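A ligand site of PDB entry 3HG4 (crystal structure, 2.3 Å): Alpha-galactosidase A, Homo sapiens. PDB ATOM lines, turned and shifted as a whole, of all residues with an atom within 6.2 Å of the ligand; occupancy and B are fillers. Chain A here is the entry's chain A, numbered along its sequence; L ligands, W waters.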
ATOM      1  N   TRP A  16      34.907  13.329 -14.745  1.00  0.00           N
ATOM      2  CA  TRP A  16      35.018  12.607 -16.028  1.00  0.00           C
ATOM      3  C   TRP A  16      36.321  12.795 -16.800  1.00  0.00           C
ATOM      4  O   TRP A  16      36.979  11.822 -17.114  1.00  0.00           O
ATOM      5  CB  TRP A  16      33.832  12.853 -16.964  1.00  0.00           C
ATOM      6  CG  TRP A  16      33.903  11.942 -18.169  1.00  0.00           C
ATOM      7  CD1 TRP A  16      34.105  12.314 -19.470  1.00  0.00           C
ATOM      8  CD2 TRP A  16      33.800  10.509 -18.167  1.00  0.00           C
ATOM      9  NE1 TRP A  16      34.116  11.192 -20.281  1.00  0.00           N
ATOM     10  CE2 TRP A  16      33.936  10.072 -19.506  1.00  0.00           C
ATOM     11  CE3 TRP A  16      33.594   9.539 -17.169  1.00  0.00           C
ATOM     12  CZ2 TRP A  16      33.884   8.714 -19.879  1.00  0.00           C
ATOM     13  CZ3 TRP A  16      33.535   8.189 -17.533  1.00  0.00           C
ATOM     14  CH2 TRP A  16      33.688   7.800 -18.882  1.00  0.00           C
ATOM     15  N   ASP A  61      30.492  11.335 -12.185  1.00  0.00           N
ATOM     16  CA  ASP A  61      30.095  11.133 -13.568  1.00  0.00           C
ATOM     17  C   ASP A  61      29.850   9.619 -13.743  1.00  0.00           C
ATOM     18  O   ASP A  61      29.473   8.953 -12.786  1.00  0.00           O
ATOM     19  CB  ASP A  61      31.168  11.704 -14.515  1.00  0.00           C
ATOM     20  CG  ASP A  61      30.620  12.041 -15.897  1.00  0.00           C
ATOM     21  OD1 ASP A  61      30.451  11.128 -16.723  1.00  0.00           O
ATOM     22  OD2 ASP A  61      30.404  13.247 -16.170  1.00  0.00           O
ATOM     23  N   ASP A  62      30.052   9.093 -14.956  1.00  0.00           N
ATOM     24  CA  ASP A  62      29.779   7.692 -15.265  1.00  0.00           C
ATOM     25  C   ASP A  62      30.695   6.746 -14.460  1.00  0.00           C
ATOM     26  O   ASP A  62      31.683   7.183 -13.872  1.00  0.00           O
ATOM     27  CB  ASP A  62      29.977   7.464 -16.770  1.00  0.00           C
ATOM     28  CG  ASP A  62      29.152   6.293 -17.333  1.00  0.00           C
ATOM     29  OD1 ASP A  62      28.756   5.357 -16.588  1.00  0.00           O
ATOM     30  OD2 ASP A  62      28.923   6.298 -18.557  1.00  0.00           O
ATOM     31  N   CYS A  63      30.332   5.463 -14.433  1.00  0.00           N
ATOM     32  CA  CYS A  63      31.137   4.388 -13.817  1.00  0.00           C
ATOM     33  C   CYS A  63      31.155   4.391 -12.289  1.00  0.00           C
ATOM     34  O   CYS A  63      32.137   3.980 -11.672  1.00  0.00           O
ATOM     35  CB  CYS A  63      32.560   4.341 -14.389  1.00  0.00           C
ATOM     36  SG  CYS A  63      32.603   4.467 -16.195  1.00  0.00           S
ATOM     37  N   TYR A 103      25.246  10.915 -11.778  1.00  0.00           N
ATOM     38  CA  TYR A 103      25.110  10.747 -13.220  1.00  0.00           C
ATOM     39  C   TYR A 103      24.190   9.567 -13.531  1.00  0.00           C
ATOM     40  O   TYR A 103      24.250   8.523 -12.880  1.00  0.00           O
ATOM     41  CB  TYR A 103      26.510  10.541 -13.837  1.00  0.00           C
ATOM     42  CG  TYR A 103      26.557  10.011 -15.263  1.00  0.00           C
ATOM     43  CD1 TYR A 103      26.928  10.828 -16.329  1.00  0.00           C
ATOM     44  CD2 TYR A 103      26.274   8.671 -15.538  1.00  0.00           C
ATOM     45  CE1 TYR A 103      26.995  10.330 -17.642  1.00  0.00           C
ATOM     46  CE2 TYR A 103      26.327   8.171 -16.846  1.00  0.00           C
ATOM     47  CZ  TYR A 103      26.691   9.016 -17.888  1.00  0.00           C
ATOM     48  OH  TYR A 103      26.736   8.519 -19.174  1.00  0.00           O
ATOM     49  N   ASP A 105      21.598   8.020 -17.250  1.00  0.00           N
ATOM     50  CA  ASP A 105      21.429   8.053 -18.704  1.00  0.00           C
ATOM     51  C   ASP A 105      19.982   7.799 -19.126  1.00  0.00           C
ATOM     52  O   ASP A 105      19.327   6.881 -18.623  1.00  0.00           O
ATOM     53  CB  ASP A 105      22.377   7.028 -19.345  1.00  0.00           C
ATOM     54  CG  ASP A 105      22.529   7.219 -20.841  1.00  0.00           C
ATOM     55  OD1 ASP A 105      23.573   7.770 -21.253  1.00  0.00           O
ATOM     56  OD2 ASP A 105      21.617   6.817 -21.601  1.00  0.00           O
ATOM     57  N   THR A 110      24.184   3.576 -19.760  1.00  0.00           N
ATOM     58  CA  THR A 110      25.070   4.742 -19.720  1.00  0.00           C
ATOM     59  C   THR A 110      26.109   4.582 -20.817  1.00  0.00           C
ATOM     60  O   THR A 110      26.279   3.489 -21.358  1.00  0.00           O
ATOM     61  CB  THR A 110      25.757   4.926 -18.341  1.00  0.00           C
ATOM     62  OG1 THR A 110      26.785   3.944 -18.168  1.00  0.00           O
ATOM     63  CG2 THR A 110      24.747   4.818 -17.196  1.00  0.00           C
ATOM     64  N   CYS A 111      26.794   5.668 -21.148  1.00  0.00           N
ATOM     65  CA  CYS A 111      27.777   5.648 -22.230  1.00  0.00           C
ATOM     66  C   CYS A 111      28.905   4.639 -21.993  1.00  0.00           C
ATOM     67  O   CYS A 111      29.424   4.056 -22.951  1.00  0.00           O
ATOM     68  CB  CYS A 111      28.342   7.044 -22.506  1.00  0.00           C
ATOM     69  SG  CYS A 111      27.093   8.248 -22.972  1.00  0.00           S
ATOM     70  N   ALA A 112      29.264   4.437 -20.738  1.00  0.00           N
ATOM     71  CA  ALA A 112      30.276   3.425 -20.387  1.00  0.00           C
ATOM     72  C   ALA A 112      29.708   2.006 -20.264  1.00  0.00           C
ATOM     73  O   ALA A 112      30.466   1.058 -20.055  1.00  0.00           O
ATOM     74  CB  ALA A 112      31.016   3.820 -19.130  1.00  0.00           C
ATOM     75  N   LYS A 137      23.454  14.794 -13.611  1.00  0.00           N
ATOM     76  CA  LYS A 137      23.873  14.844 -15.005  1.00  0.00           C
ATOM     77  C   LYS A 137      23.231  13.672 -15.740  1.00  0.00           C
ATOM     78  O   LYS A 137      23.417  12.511 -15.358  1.00  0.00           O
ATOM     79  CB  LYS A 137      25.400  14.788 -15.118  1.00  0.00           C
ATOM     80  CG  LYS A 137      25.935  15.056 -16.521  1.00  0.00           C
ATOM     81  CD  LYS A 137      27.437  14.878 -16.605  1.00  0.00           C
ATOM     82  CE  LYS A 137      27.878  14.748 -18.059  1.00  0.00           C
ATOM     83  NZ  LYS A 137      29.357  14.647 -18.166  1.00  0.00           N
ATOM     84  N   ASP A 139      22.972  11.855 -19.141  1.00  0.00           N
ATOM     85  CA  ASP A 139      23.566  11.627 -20.462  1.00  0.00           C
ATOM     86  C   ASP A 139      22.583  10.989 -21.479  1.00  0.00           C
ATOM     87  O   ASP A 139      21.536  10.452 -21.093  1.00  0.00           O
ATOM     88  CB  ASP A 139      24.823  10.762 -20.318  1.00  0.00           C
ATOM     89  CG  ASP A 139      25.920  11.136 -21.307  1.00  0.00           C
ATOM     90  OD1 ASP A 139      25.614  11.744 -22.364  1.00  0.00           O
ATOM     91  OD2 ASP A 139      27.083  10.804 -21.032  1.00  0.00           O
ATOM     92  N   GLY A 140      22.933  11.056 -22.767  1.00  0.00           N
ATOM     93  CA  GLY A 140      22.025  10.648 -23.840  1.00  0.00           C
ATOM     94  C   GLY A 140      22.335   9.404 -24.652  1.00  0.00           C
ATOM     95  O   GLY A 140      21.693   9.175 -25.687  1.00  0.00           O
ATOM     96  N   CYS A 141      23.283   8.579 -24.202  1.00  0.00           N
ATOM     97  CA  CYS A 141      23.648   7.349 -24.922  1.00  0.00           C
ATOM     98  C   CYS A 141      22.565   6.280 -24.943  1.00  0.00           C
ATOM     99  O   CYS A 141      21.646   6.296 -24.125  1.00  0.00           O
ATOM    100  CB  CYS A 141      24.935   6.748 -24.359  1.00  0.00           C
ATOM    101  SG  CYS A 141      26.413   7.648 -24.777  1.00  0.00           S
ATOM    102  N   GLU A 172      22.092  16.298 -21.513  1.00  0.00           N
ATOM    103  CA  GLU A 172      22.858  16.146 -22.759  1.00  0.00           C
ATOM    104  C   GLU A 172      21.929  16.101 -23.960  1.00  0.00           C
ATOM    105  O   GLU A 172      22.334  15.725 -25.066  1.00  0.00           O
ATOM    106  CB  GLU A 172      23.762  14.913 -22.706  1.00  0.00           C
ATOM    107  CG  GLU A 172      25.121  15.172 -22.070  1.00  0.00           C
ATOM    108  CD  GLU A 172      24.994  15.543 -20.600  1.00  0.00           C
ATOM    109  OE1 GLU A 172      24.821  14.633 -19.772  1.00  0.00           O
ATOM    110  OE2 GLU A 172      25.071  16.746 -20.284  1.00  0.00           O
ATOM    111  N   LEU A 175      22.857  17.807 -27.585  1.00  0.00           N
ATOM    112  CA  LEU A 175      23.999  17.095 -28.155  1.00  0.00           C
ATOM    113  C   LEU A 175      23.594  15.794 -28.874  1.00  0.00           C
ATOM    114  O   LEU A 175      24.063  15.526 -29.990  1.00  0.00           O
ATOM    115  CB  LEU A 175      25.047  16.789 -27.070  1.00  0.00           C
ATOM    116  CG  LEU A 175      26.200  15.812 -27.350  1.00  0.00           C
ATOM    117  CD1 LEU A 175      27.176  16.377 -28.372  1.00  0.00           C
ATOM    118  CD2 LEU A 175      26.924  15.482 -26.054  1.00  0.00           C
ATOM    119  N   TYR A 176      22.729  15.010 -28.243  1.00  0.00           N
ATOM    120  CA  TYR A 176      22.291  13.728 -28.808  1.00  0.00           C
ATOM    121  C   TYR A 176      21.131  13.838 -29.787  1.00  0.00           C
ATOM    122  O   TYR A 176      20.813  12.885 -30.488  1.00  0.00           O
ATOM    123  CB  TYR A 176      22.008  12.702 -27.708  1.00  0.00           C
ATOM    124  CG  TYR A 176      23.283  12.236 -27.038  1.00  0.00           C
ATOM    125  CD1 TYR A 176      24.004  11.158 -27.545  1.00  0.00           C
ATOM    126  CD2 TYR A 176      23.793  12.915 -25.931  1.00  0.00           C
ATOM    127  CE1 TYR A 176      25.194  10.746 -26.941  1.00  0.00           C
ATOM    128  CE2 TYR A 176      24.974  12.508 -25.328  1.00  0.00           C
ATOM    129  CZ  TYR A 176      25.671  11.428 -25.839  1.00  0.00           C
ATOM    130  OH  TYR A 176      26.846  11.031 -25.249  1.00  0.00           O
ATOM    131  N   ARG A 196      24.305  20.367 -22.512  1.00  0.00           N
ATOM    132  CA  ARG A 196      25.496  20.203 -23.337  1.00  0.00           C
ATOM    133  C   ARG A 196      25.098  20.261 -24.803  1.00  0.00           C
ATOM    134  O   ARG A 196      24.234  19.498 -25.246  1.00  0.00           O
ATOM    135  CB  ARG A 196      26.191  18.884 -22.988  1.00  0.00           C
ATOM    136  CG  ARG A 196      27.042  18.932 -21.695  1.00  0.00           C
ATOM    137  CD  ARG A 196      28.513  19.339 -21.975  1.00  0.00           C
ATOM    138  NE  ARG A 196      29.029  18.656 -23.167  1.00  0.00           N
ATOM    139  CZ  ARG A 196      29.482  17.405 -23.192  1.00  0.00           C
ATOM    140  NH1 ARG A 196      29.498  16.676 -22.081  1.00  0.00           N
ATOM    141  NH2 ARG A 196      29.909  16.868 -24.342  1.00  0.00           N
ATOM    142  N   ASP A 200      32.328  16.050 -26.257  1.00  0.00           N
ATOM    143  CA  ASP A 200      33.142  16.015 -25.022  1.00  0.00           C
ATOM    144  C   ASP A 200      34.448  16.773 -25.166  1.00  0.00           C
ATOM    145  O   ASP A 200      35.190  16.575 -26.128  1.00  0.00           O
ATOM    146  CB  ASP A 200      33.471  14.563 -24.631  1.00  0.00           C
ATOM    147  CG  ASP A 200      32.239  13.729 -24.324  1.00  0.00           C
ATOM    148  OD1 ASP A 200      31.097  14.234 -24.428  1.00  0.00           O
ATOM    149  OD2 ASP A 200      32.429  12.537 -23.975  1.00  0.00           O
ATOM    150  N   ASP A 235      30.996  22.294 -21.584  1.00  0.00           N
ATOM    151  CA  ASP A 235      31.747  21.205 -20.907  1.00  0.00           C
ATOM    152  C   ASP A 235      32.759  21.694 -19.854  1.00  0.00           C
ATOM    153  O   ASP A 235      32.870  22.896 -19.578  1.00  0.00           O
ATOM    154  CB  ASP A 235      32.371  20.206 -21.900  1.00  0.00           C
ATOM    155  CG  ASP A 235      32.344  18.776 -21.371  1.00  0.00           C
ATOM    156  OD1 ASP A 235      31.927  18.574 -20.205  1.00  0.00           O
ATOM    157  OD2 ASP A 235      32.735  17.869 -22.117  1.00  0.00           O
ATOM    158  N   MET A 236      33.477  20.728 -19.270  1.00  0.00           N
ATOM    159  CA  MET A 236      34.307  20.942 -18.097  1.00  0.00           C
ATOM    160  C   MET A 236      35.494  21.875 -18.332  1.00  0.00           C
ATOM    161  O   MET A 236      36.023  21.950 -19.445  1.00  0.00           O
ATOM    162  CB  MET A 236      34.839  19.597 -17.583  1.00  0.00           C
ATOM    163  CG  MET A 236      33.779  18.657 -17.036  1.00  0.00           C
ATOM    164  SD  MET A 236      34.311  16.926 -17.078  1.00  0.00           S
ATOM    165  CE  MET A 236      34.171  16.558 -18.826  1.00  0.00           C
HETATM  166  F1  LIG L   1      28.008  13.452 -20.943  1.00  0.00           F
HETATM  167  C1  LIG L   1      28.722  12.683 -21.745  1.00  0.00           C
HETATM  168  F2  LIG L   1      28.607  13.106 -23.005  1.00  0.00           F
HETATM  169  C2  LIG L   1      28.212  11.245 -21.618  1.00  0.00           C
HETATM  170  C3  LIG L   1      30.192  12.778 -21.313  1.00  0.00           C
HETATM  171  O1  LIG L   1      30.491  14.100 -20.829  1.00  0.00           O
HETATM  172  C4  LIG L   1      30.531  11.710 -20.259  1.00  0.00           C
HETATM  173  O2  LIG L   1      29.754  11.903 -19.069  1.00  0.00           O
HETATM  174  C5  LIG L   1      30.309  10.301 -20.805  1.00  0.00           C
HETATM  175  O3  LIG L   1      29.246  10.261 -21.772  1.00  0.00           O
HETATM  176  C6  LIG L   1      30.035   9.290 -19.690  1.00  0.00           C
HETATM  177  O4  LIG L   1      30.200   7.951 -20.151  1.00  0.00           O
HETATM  178  O   HOH W   1      31.706   6.776 -22.102  1.00  0.00           O
HETATM  179  O   HOH W   2      29.147  12.372 -25.620  1.00  0.00           O
HETATM  180  O   HOH W   3      32.774  15.354 -21.447  1.00  0.00           O
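OD2 of Asp 139 is covalently linked to C2 of the ligand, 1.3 Å away. OD1 of Asp 61 sits at hydrogen-bond distance from O2 of the ligand, at 2.6 Å. An oxygen (O4) of the ligand is in hydrogen-bond range of the side-chain carboxylate of Asp 62. O2 of the ligand lies within hydrogen-bond range of NZ of Lys 137 (2.9 Å). NH1 of Arg 196 lies within hydrogen-bond range of O1 of the ligand, 3.0 Å away.
SG of Cys 111 lies close to O3 of the ligand (3.2 Å). OD1 of Asp 200 lies close to F2 of the ligand (3.1 Å). NE1 of Trp 16 touches C4 of the ligand (3.6 Å). OH of Tyr 103 touches C6 of the ligand (3.4 Å). Ala 112 touches the ligand (N to O4, 3.7 Å). Glu 172 touches the ligand. OH of Tyr 176 touches F2 of the ligand (3.5 Å). Hydrophobic or aromatic side chains within 4 Å of the ligand: Trp 16 and Tyr 103. Of the 20 residues printed, 12 come within 4 Å of the ligand.
The side-chain carboxylate (OD1) of Asp 139 lies close to the side-chain hydroxyl (OH) of Tyr 176 (3.2 Å). The side-chain carboxylate (OD2) of Asp 61 is in salt-bridge range of the side-chain amino group (NZ) of Lys 137, at 2.7 Å. The backbone NH (N) of Ala 112 lies within hydrogen-bond range of the side-chain carboxylate (OD2) of Asp 62. OG1 of Thr 110 lies within hydrogen-bond range of OD1 of Asp 62, at 2.9 Å. The guanidinium group (NH2) of Arg 196 is in salt-bridge range of the side-chain carboxylate (OD1) of Asp 200. The backbone NH (N) of Cys 111 is in hydrogen-bond range of the side-chain hydroxyl (OH) of Tyr 103, 3.5 Å away. SG of Cys 141 is disulfide-bonded to SG of Cys 111 (2.0 Å). The side-chain sulfur (SG) of Cys 141 sits at hydrogen-bond distance from the side-chain hydroxyl (OH) of Tyr 176, 3.4 Å away.
Water W3 lies within hydrogen-bond range of the side-chain carboxylate (OD2) of Asp 235 (2.6 Å) and an oxygen (O1) of the ligand (2.7 Å). Water W2 lies within hydrogen-bond range of the side-chain hydroxyl of Tyr 176 and the side-chain carboxylate of Asp 200.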
